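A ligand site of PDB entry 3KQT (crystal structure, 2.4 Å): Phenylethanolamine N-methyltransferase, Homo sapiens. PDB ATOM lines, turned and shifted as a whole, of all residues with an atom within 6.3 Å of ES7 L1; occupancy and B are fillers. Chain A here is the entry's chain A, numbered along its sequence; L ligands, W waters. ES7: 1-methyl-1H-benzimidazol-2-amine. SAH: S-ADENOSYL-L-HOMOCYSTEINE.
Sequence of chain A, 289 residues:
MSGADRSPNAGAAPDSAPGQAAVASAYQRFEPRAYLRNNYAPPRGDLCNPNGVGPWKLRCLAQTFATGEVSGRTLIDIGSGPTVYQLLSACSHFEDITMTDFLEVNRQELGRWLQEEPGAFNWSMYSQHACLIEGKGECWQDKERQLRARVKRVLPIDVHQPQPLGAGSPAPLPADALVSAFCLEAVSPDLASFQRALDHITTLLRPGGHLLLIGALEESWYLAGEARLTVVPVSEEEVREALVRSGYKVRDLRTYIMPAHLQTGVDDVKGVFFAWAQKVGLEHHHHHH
The side-chain amide nitrogen (ND2) of Asn 39 sits at hydrogen-bond distance from the backbone carbonyl oxygen (O) of Tyr 35, 3.0 Å away. The side-chain hydroxyl of Tyr 85 lies within hydrogen-bond range of the side-chain hydroxyl of Tyr 40 (3.4 Å). The guanidinium group of Arg 44 lies within hydrogen-bond range of the side-chain amide oxygen of Asn 39 (3.1 Å). The guanidinium group of Arg 44 is in salt-bridge range of the side-chain carboxylate of Asp 267 (2.8 Å). The guanidinium group (NE) of Arg 44 lies within hydrogen-bond range of the backbone carbonyl oxygen (O) of Leu 262. The side-chain carboxylate (OD1) of Asp 267 sits close to the backbone NH (N) of Val 269.
OH of Tyr 35 sits at hydrogen-bond distance from N11 of ES7 L1, 2.7 Å away. N09 of ES7 L1 lies within hydrogen-bond range of OH of Tyr 40, 3.0 Å away. The side-chain hydroxyl (OH) of Tyr 35 is in hydrogen-bond range of an oxygen (OXT) of SAH L2 (2.5 Å). OH of Tyr 40 sits at hydrogen-bond distance from OXT of SAH L2, 2.5 Å away. OH of Tyr 85 is in hydrogen-bond range of O of SAH L2 (2.9 Å). The backbone carbonyl oxygen of Ala 181 is in hydrogen-bond range of a nitrogen (N) of SAH L2.
Merely in contact with ES7 L1: Phe 182, Arg 44, Lys 57, Val 53, Asn 39, Glu 219 and Asp 267. Hydrophobic or aromatic side chains within 4 Å of ES7 L1: Tyr 35, Tyr 40, Val 53 and Phe 182. Of the 21 residues printed, 9 come within 4 Å of ES7 L1.
Water W1 lies within hydrogen-bond range of N11 of ES7 L1 (2.8 Å), O of Phe 182 (3.4 Å) and SD of SAH L2 (3.7 Å). Water W2 lies within hydrogen-bond range of OE1 of Glu 219 and N11 of ES7 L1.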
ATOM      1  N   TYR A  35     -27.165 -20.443  22.162  1.00  0.00           N
ATOM      2  CA  TYR A  35     -26.159 -19.411  22.008  1.00  0.00           C
ATOM      3  C   TYR A  35     -26.736 -18.188  21.269  1.00  0.00           C
ATOM      4  O   TYR A  35     -26.564 -17.045  21.698  1.00  0.00           O
ATOM      5  CB  TYR A  35     -24.913 -19.959  21.282  1.00  0.00           C
ATOM      6  CG  TYR A  35     -23.883 -18.886  20.989  1.00  0.00           C
ATOM      7  CD1 TYR A  35     -23.054 -18.377  21.988  1.00  0.00           C
ATOM      8  CD2 TYR A  35     -23.746 -18.362  19.700  1.00  0.00           C
ATOM      9  CE1 TYR A  35     -22.120 -17.384  21.705  1.00  0.00           C
ATOM     10  CE2 TYR A  35     -22.809 -17.386  19.416  1.00  0.00           C
ATOM     11  CZ  TYR A  35     -22.008 -16.893  20.420  1.00  0.00           C
ATOM     12  OH  TYR A  35     -21.092 -15.914  20.132  1.00  0.00           O
ATOM     13  N   ASN A  39     -27.397 -14.279  22.815  1.00  0.00           N
ATOM     14  CA  ASN A  39     -26.546 -13.189  22.366  1.00  0.00           C
ATOM     15  C   ASN A  39     -27.095 -12.358  21.209  1.00  0.00           C
ATOM     16  O   ASN A  39     -26.651 -11.235  20.996  1.00  0.00           O
ATOM     17  CB  ASN A  39     -25.143 -13.700  22.020  1.00  0.00           C
ATOM     18  CG  ASN A  39     -24.445 -14.339  23.201  1.00  0.00           C
ATOM     19  OD1 ASN A  39     -23.989 -13.654  24.106  1.00  0.00           O
ATOM     20  ND2 ASN A  39     -24.380 -15.664  23.202  1.00  0.00           N
ATOM     21  N   TYR A  40     -28.058 -12.892  20.476  1.00  0.00           N
ATOM     22  CA  TYR A  40     -28.522 -12.220  19.264  1.00  0.00           C
ATOM     23  C   TYR A  40     -30.043 -12.084  19.194  1.00  0.00           C
ATOM     24  O   TYR A  40     -30.583 -11.738  18.145  1.00  0.00           O
ATOM     25  CB  TYR A  40     -27.940 -12.906  18.036  1.00  0.00           C
ATOM     26  CG  TYR A  40     -26.435 -12.954  18.143  1.00  0.00           C
ATOM     27  CD1 TYR A  40     -25.787 -14.096  18.584  1.00  0.00           C
ATOM     28  CD2 TYR A  40     -25.673 -11.825  17.881  1.00  0.00           C
ATOM     29  CE1 TYR A  40     -24.423 -14.120  18.715  1.00  0.00           C
ATOM     30  CE2 TYR A  40     -24.315 -11.849  17.999  1.00  0.00           C
ATOM     31  CZ  TYR A  40     -23.687 -12.998  18.418  1.00  0.00           C
ATOM     32  OH  TYR A  40     -22.325 -12.998  18.533  1.00  0.00           O
ATOM     33  N   ARG A  44     -29.884  -8.074  23.792  1.00  0.00           N
ATOM     34  CA  ARG A  44     -28.621  -7.882  23.068  1.00  0.00           C
ATOM     35  C   ARG A  44     -28.817  -7.825  21.574  1.00  0.00           C
ATOM     36  O   ARG A  44     -28.011  -7.230  20.865  1.00  0.00           O
ATOM     37  CB  ARG A  44     -27.608  -8.985  23.411  1.00  0.00           C
ATOM     38  CG  ARG A  44     -27.022  -8.836  24.816  1.00  0.00           C
ATOM     39  CD  ARG A  44     -26.037  -9.937  25.142  1.00  0.00           C
ATOM     40  NE  ARG A  44     -25.520  -9.790  26.501  1.00  0.00           N
ATOM     41  CZ  ARG A  44     -24.494 -10.466  26.989  1.00  0.00           C
ATOM     42  NH1 ARG A  44     -23.856 -11.334  26.210  1.00  0.00           N
ATOM     43  NH2 ARG A  44     -24.092 -10.272  28.231  1.00  0.00           N
ATOM     44  N   VAL A  53     -25.122  -2.810  21.916  1.00  0.00           N
ATOM     45  CA  VAL A  53     -23.911  -3.466  21.439  1.00  0.00           C
ATOM     46  C   VAL A  53     -24.007  -3.934  19.985  1.00  0.00           C
ATOM     47  O   VAL A  53     -23.008  -3.947  19.262  1.00  0.00           O
ATOM     48  CB  VAL A  53     -23.524  -4.675  22.329  1.00  0.00           C
ATOM     49  CG1 VAL A  53     -24.528  -5.822  22.151  1.00  0.00           C
ATOM     50  CG2 VAL A  53     -22.115  -5.139  22.002  1.00  0.00           C
ATOM     51  N   GLY A  54     -25.201  -4.346  19.556  1.00  0.00           N
ATOM     52  CA  GLY A  54     -25.381  -4.821  18.199  1.00  0.00           C
ATOM     53  C   GLY A  54     -25.049  -3.755  17.165  1.00  0.00           C
ATOM     54  O   GLY A  54     -24.261  -3.988  16.236  1.00  0.00           O
ATOM     55  N   LYS A  57     -21.201  -2.936  17.108  1.00  0.00           N
ATOM     56  CA  LYS A  57     -20.392  -3.883  16.333  1.00  0.00           C
ATOM     57  C   LYS A  57     -20.546  -3.672  14.823  1.00  0.00           C
ATOM     58  O   LYS A  57     -19.547  -3.592  14.114  1.00  0.00           O
ATOM     59  CB  LYS A  57     -20.732  -5.332  16.689  1.00  0.00           C
ATOM     60  CG  LYS A  57     -20.476  -5.683  18.158  1.00  0.00           C
ATOM     61  CD  LYS A  57     -20.353  -7.186  18.372  1.00  0.00           C
ATOM     62  CE  LYS A  57     -21.591  -7.955  17.916  1.00  0.00           C
ATOM     63  NZ  LYS A  57     -22.689  -7.980  18.919  1.00  0.00           N
ATOM     64  N   TYR A  85     -23.665 -12.098  11.108  1.00  0.00           N
ATOM     65  CA  TYR A  85     -23.714 -10.637  11.216  1.00  0.00           C
ATOM     66  C   TYR A  85     -22.335 -10.046  10.986  1.00  0.00           C
ATOM     67  O   TYR A  85     -22.206  -8.916  10.519  1.00  0.00           O
ATOM     68  CB  TYR A  85     -24.211 -10.193  12.604  1.00  0.00           C
ATOM     69  CG  TYR A  85     -23.180 -10.441  13.682  1.00  0.00           C
ATOM     70  CD1 TYR A  85     -22.271  -9.442  14.029  1.00  0.00           C
ATOM     71  CD2 TYR A  85     -23.092 -11.666  14.334  1.00  0.00           C
ATOM     72  CE1 TYR A  85     -21.302  -9.665  15.011  1.00  0.00           C
ATOM     73  CE2 TYR A  85     -22.128 -11.901  15.310  1.00  0.00           C
ATOM     74  CZ  TYR A  85     -21.240 -10.892  15.637  1.00  0.00           C
ATOM     75  OH  TYR A  85     -20.289 -11.128  16.588  1.00  0.00           O
ATOM     76  N   TYR A 126     -30.461  -7.567  11.624  1.00  0.00           N
ATOM     77  CA  TYR A 126     -29.047  -7.205  11.492  1.00  0.00           C
ATOM     78  C   TYR A 126     -28.737  -6.774  10.062  1.00  0.00           C
ATOM     79  O   TYR A 126     -27.979  -5.824   9.837  1.00  0.00           O
ATOM     80  CB  TYR A 126     -28.148  -8.383  11.911  1.00  0.00           C
ATOM     81  CG  TYR A 126     -28.027  -8.569  13.412  1.00  0.00           C
ATOM     82  CD1 TYR A 126     -28.988  -9.276  14.131  1.00  0.00           C
ATOM     83  CD2 TYR A 126     -26.934  -8.071  14.104  1.00  0.00           C
ATOM     84  CE1 TYR A 126     -28.867  -9.461  15.513  1.00  0.00           C
ATOM     85  CE2 TYR A 126     -26.805  -8.254  15.475  1.00  0.00           C
ATOM     86  CZ  TYR A 126     -27.776  -8.944  16.182  1.00  0.00           C
ATOM     87  OH  TYR A 126     -27.641  -9.109  17.542  1.00  0.00           O
ATOM     88  N   ALA A 181     -14.845 -13.224  15.280  1.00  0.00           N
ATOM     89  CA  ALA A 181     -15.589 -12.583  16.345  1.00  0.00           C
ATOM     90  C   ALA A 181     -15.895 -13.534  17.491  1.00  0.00           C
ATOM     91  O   ALA A 181     -16.529 -14.564  17.299  1.00  0.00           O
ATOM     92  CB  ALA A 181     -16.888 -11.969  15.807  1.00  0.00           C
ATOM     93  N   PHE A 182     -15.439 -13.153  18.687  1.00  0.00           N
ATOM     94  CA  PHE A 182     -15.740 -13.887  19.913  1.00  0.00           C
ATOM     95  C   PHE A 182     -15.233 -15.327  19.876  1.00  0.00           C
ATOM     96  O   PHE A 182     -15.839 -16.206  20.482  1.00  0.00           O
ATOM     97  CB  PHE A 182     -17.235 -13.878  20.197  1.00  0.00           C
ATOM     98  CG  PHE A 182     -17.795 -12.504  20.419  1.00  0.00           C
ATOM     99  CD1 PHE A 182     -18.696 -11.959  19.524  1.00  0.00           C
ATOM    100  CD2 PHE A 182     -17.417 -11.760  21.513  1.00  0.00           C
ATOM    101  CE1 PHE A 182     -19.216 -10.700  19.728  1.00  0.00           C
ATOM    102  CE2 PHE A 182     -17.923 -10.493  21.727  1.00  0.00           C
ATOM    103  CZ  PHE A 182     -18.830  -9.961  20.826  1.00  0.00           C
ATOM    104  N   GLU A 185     -10.538 -15.651  22.392  1.00  0.00           N
ATOM    105  CA  GLU A 185     -10.601 -15.594  23.847  1.00  0.00           C
ATOM    106  C   GLU A 185     -11.508 -16.693  24.411  1.00  0.00           C
ATOM    107  O   GLU A 185     -11.309 -17.178  25.515  1.00  0.00           O
ATOM    108  CB  GLU A 185     -11.038 -14.192  24.331  1.00  0.00           C
ATOM    109  CG  GLU A 185     -12.532 -13.859  24.157  1.00  0.00           C
ATOM    110  CD  GLU A 185     -12.913 -13.414  22.742  1.00  0.00           C
ATOM    111  OE1 GLU A 185     -12.101 -13.525  21.813  1.00  0.00           O
ATOM    112  OE2 GLU A 185     -14.068 -12.957  22.569  1.00  0.00           O
ATOM    113  N   GLY A 215     -14.049  -9.204  19.993  1.00  0.00           N
ATOM    114  CA  GLY A 215     -13.911 -10.096  21.113  1.00  0.00           C
ATOM    115  C   GLY A 215     -14.483  -9.547  22.402  1.00  0.00           C
ATOM    116  O   GLY A 215     -14.778  -8.352  22.503  1.00  0.00           O
ATOM    117  N   ALA A 216     -14.639 -10.430  23.376  1.00  0.00           N
ATOM    118  CA  ALA A 216     -15.137 -10.040  24.679  1.00  0.00           C
ATOM    119  C   ALA A 216     -13.984  -9.590  25.563  1.00  0.00           C
ATOM    120  O   ALA A 216     -12.896 -10.185  25.527  1.00  0.00           O
ATOM    121  CB  ALA A 216     -15.890 -11.195  25.325  1.00  0.00           C
ATOM    122  N   GLU A 219     -14.019 -11.308  30.109  1.00  0.00           N
ATOM    123  CA  GLU A 219     -15.030 -12.352  30.258  1.00  0.00           C
ATOM    124  C   GLU A 219     -14.336 -13.623  30.725  1.00  0.00           C
ATOM    125  O   GLU A 219     -13.202 -13.891  30.319  1.00  0.00           O
ATOM    126  CB  GLU A 219     -15.763 -12.604  28.929  1.00  0.00           C
ATOM    127  CG  GLU A 219     -16.748 -13.772  28.956  1.00  0.00           C
ATOM    128  CD  GLU A 219     -17.356 -14.114  27.582  1.00  0.00           C
ATOM    129  OE1 GLU A 219     -18.550 -14.490  27.532  1.00  0.00           O
ATOM    130  OE2 GLU A 219     -16.650 -14.003  26.561  1.00  0.00           O
ATOM    131  N   TYR A 222     -19.303 -18.239  29.685  1.00  0.00           N
ATOM    132  CA  TYR A 222     -20.635 -18.016  29.131  1.00  0.00           C
ATOM    133  C   TYR A 222     -21.355 -19.328  28.932  1.00  0.00           C
ATOM    134  O   TYR A 222     -20.742 -20.404  28.962  1.00  0.00           O
ATOM    135  CB  TYR A 222     -20.572 -17.238  27.818  1.00  0.00           C
ATOM    136  CG  TYR A 222     -19.996 -18.012  26.665  1.00  0.00           C
ATOM    137  CD1 TYR A 222     -20.839 -18.518  25.674  1.00  0.00           C
ATOM    138  CD2 TYR A 222     -18.635 -18.237  26.540  1.00  0.00           C
ATOM    139  CE1 TYR A 222     -20.336 -19.219  24.596  1.00  0.00           C
ATOM    140  CE2 TYR A 222     -18.117 -18.942  25.455  1.00  0.00           C
ATOM    141  CZ  TYR A 222     -18.972 -19.428  24.485  1.00  0.00           C
ATOM    142  OH  TYR A 222     -18.500 -20.116  23.406  1.00  0.00           O
ATOM    143  N   MET A 258     -20.003  -2.579  28.362  1.00  0.00           N
ATOM    144  CA  MET A 258     -21.280  -3.283  28.392  1.00  0.00           C
ATOM    145  C   MET A 258     -22.216  -2.640  29.427  1.00  0.00           C
ATOM    146  O   MET A 258     -21.894  -2.601  30.610  1.00  0.00           O
ATOM    147  CB  MET A 258     -21.023  -4.770  28.687  1.00  0.00           C
ATOM    148  CG  MET A 258     -22.081  -5.774  28.226  1.00  0.00           C
ATOM    149  SD  MET A 258     -22.172  -6.099  26.450  1.00  0.00           S
ATOM    150  CE  MET A 258     -20.656  -5.373  25.864  1.00  0.00           C
ATOM    151  N   LEU A 262     -27.674  -4.957  29.404  1.00  0.00           N
ATOM    152  CA  LEU A 262     -27.253  -6.046  28.526  1.00  0.00           C
ATOM    153  C   LEU A 262     -26.388  -7.090  29.259  1.00  0.00           C
ATOM    154  O   LEU A 262     -25.839  -7.998  28.645  1.00  0.00           O
ATOM    155  CB  LEU A 262     -26.499  -5.518  27.305  1.00  0.00           C
ATOM    156  CG  LEU A 262     -27.187  -4.523  26.381  1.00  0.00           C
ATOM    157  CD1 LEU A 262     -26.209  -4.142  25.273  1.00  0.00           C
ATOM    158  CD2 LEU A 262     -28.468  -5.091  25.785  1.00  0.00           C
ATOM    159  N   ASP A 267     -23.530 -14.728  30.663  1.00  0.00           N
ATOM    160  CA  ASP A 267     -22.077 -14.660  30.763  1.00  0.00           C
ATOM    161  C   ASP A 267     -21.675 -13.554  31.735  1.00  0.00           C
ATOM    162  O   ASP A 267     -22.531 -13.028  32.463  1.00  0.00           O
ATOM    163  CB  ASP A 267     -21.437 -14.445  29.385  1.00  0.00           C
ATOM    164  CG  ASP A 267     -21.901 -13.149  28.714  1.00  0.00           C
ATOM    165  OD1 ASP A 267     -22.064 -12.127  29.425  1.00  0.00           O
ATOM    166  OD2 ASP A 267     -22.090 -13.147  27.479  1.00  0.00           O
ATOM    167  N   VAL A 269     -19.358 -10.991  30.497  1.00  0.00           N
ATOM    168  CA  VAL A 269     -18.583 -10.089  29.655  1.00  0.00           C
ATOM    169  C   VAL A 269     -18.677  -8.662  30.213  1.00  0.00           C
ATOM    170  O   VAL A 269     -19.746  -8.222  30.654  1.00  0.00           O
ATOM    171  CB  VAL A 269     -19.018 -10.157  28.166  1.00  0.00           C
ATOM    172  CG1 VAL A 269     -20.506  -9.978  28.039  1.00  0.00           C
ATOM    173  CG2 VAL A 269     -18.292  -9.123  27.330  1.00  0.00           C
ATOM    174  N   VAL A 272     -16.836  -5.139  24.930  1.00  0.00           N
ATOM    175  CA  VAL A 272     -16.500  -5.743  23.649  1.00  0.00           C
ATOM    176  C   VAL A 272     -15.435  -4.889  22.987  1.00  0.00           C
ATOM    177  O   VAL A 272     -15.516  -3.663  23.020  1.00  0.00           O
ATOM    178  CB  VAL A 272     -17.731  -5.845  22.718  1.00  0.00           C
ATOM    179  CG1 VAL A 272     -17.337  -6.384  21.384  1.00  0.00           C
ATOM    180  CG2 VAL A 272     -18.820  -6.719  23.354  1.00  0.00           C
HETATM  181  C10 ES7 L   1     -20.786 -13.122  22.329  1.00  0.00           C
HETATM  182  C01 ES7 L   1     -19.642 -12.393  24.518  1.00  0.00           C
HETATM  183  N02 ES7 L   1     -20.579 -12.227  23.387  1.00  0.00           N
HETATM  184  C03 ES7 L   1     -21.405 -11.131  23.171  1.00  0.00           C
HETATM  185  C04 ES7 L   1     -21.616  -9.915  23.934  1.00  0.00           C
HETATM  186  C05 ES7 L   1     -22.570  -8.919  23.476  1.00  0.00           C
HETATM  187  C06 ES7 L   1     -23.305  -9.149  22.250  1.00  0.00           C
HETATM  188  C07 ES7 L   1     -23.096 -10.360  21.496  1.00  0.00           C
HETATM  189  C08 ES7 L   1     -22.142 -11.356  21.955  1.00  0.00           C
HETATM  190  N09 ES7 L   1     -21.756 -12.554  21.444  1.00  0.00           N
HETATM  191  N11 ES7 L   1     -20.118 -14.383  22.161  1.00  0.00           N
HETATM  192  N   SAH L   2     -18.180 -15.940  15.520  1.00  0.00           N
HETATM  193  CA  SAH L   2     -19.404 -16.210  16.274  1.00  0.00           C
HETATM  194  CB  SAH L   2     -19.179 -17.386  17.260  1.00  0.00           C
HETATM  195  CG  SAH L   2     -18.628 -16.900  18.620  1.00  0.00           C
HETATM  196  SD  SAH L   2     -18.640 -18.261  19.848  1.00  0.00           S
HETATM  197  C   SAH L   2     -19.858 -14.943  17.015  1.00  0.00           C
HETATM  198  O   SAH L   2     -19.508 -13.876  16.621  1.00  0.00           O
HETATM  199  OXT SAH L   2     -21.023 -15.027  17.761  1.00  0.00           O
HETATM  200  C5' SAH L   2     -17.018 -19.079  19.840  1.00  0.00           C
HETATM  201  C4' SAH L   2     -16.896 -20.056  18.659  1.00  0.00           C
HETATM  202  O4' SAH L   2     -15.578 -20.690  18.587  1.00  0.00           O
HETATM  203  C3' SAH L   2     -17.944 -21.186  18.677  1.00  0.00           C
HETATM  204  O3' SAH L   2     -18.595 -21.203  17.429  1.00  0.00           O
HETATM  205  C2' SAH L   2     -17.066 -22.404  18.821  1.00  0.00           C
HETATM  206  O2' SAH L   2     -17.606 -23.641  18.428  1.00  0.00           O
HETATM  207  C1' SAH L   2     -15.821 -22.024  18.039  1.00  0.00           C
HETATM  208  N9  SAH L   2     -14.761 -22.909  18.481  1.00  0.00           N
HETATM  209  C8  SAH L   2     -14.797 -23.776  19.687  1.00  0.00           C
HETATM  210  N7  SAH L   2     -13.500 -24.428  19.776  1.00  0.00           N
HETATM  211  C5  SAH L   2     -12.662 -23.969  18.658  1.00  0.00           C
HETATM  212  C6  SAH L   2     -11.247 -24.292  18.247  1.00  0.00           C
HETATM  213  N6  SAH L   2     -10.441 -25.208  19.047  1.00  0.00           N
HETATM  214  N1  SAH L   2     -10.682 -23.661  17.065  1.00  0.00           N
HETATM  215  C2  SAH L   2     -11.497 -22.686  16.252  1.00  0.00           C
HETATM  216  N3  SAH L   2     -12.896 -22.366  16.655  1.00  0.00           N
HETATM  217  C4  SAH L   2     -13.461 -23.004  17.854  1.00  0.00           C
HETATM  218  O   HOH W   1     -18.182 -16.290  22.887  1.00  0.00           O
HETATM  219  O   HOH W   2     -19.355 -15.261  25.079  1.00  0.00           O
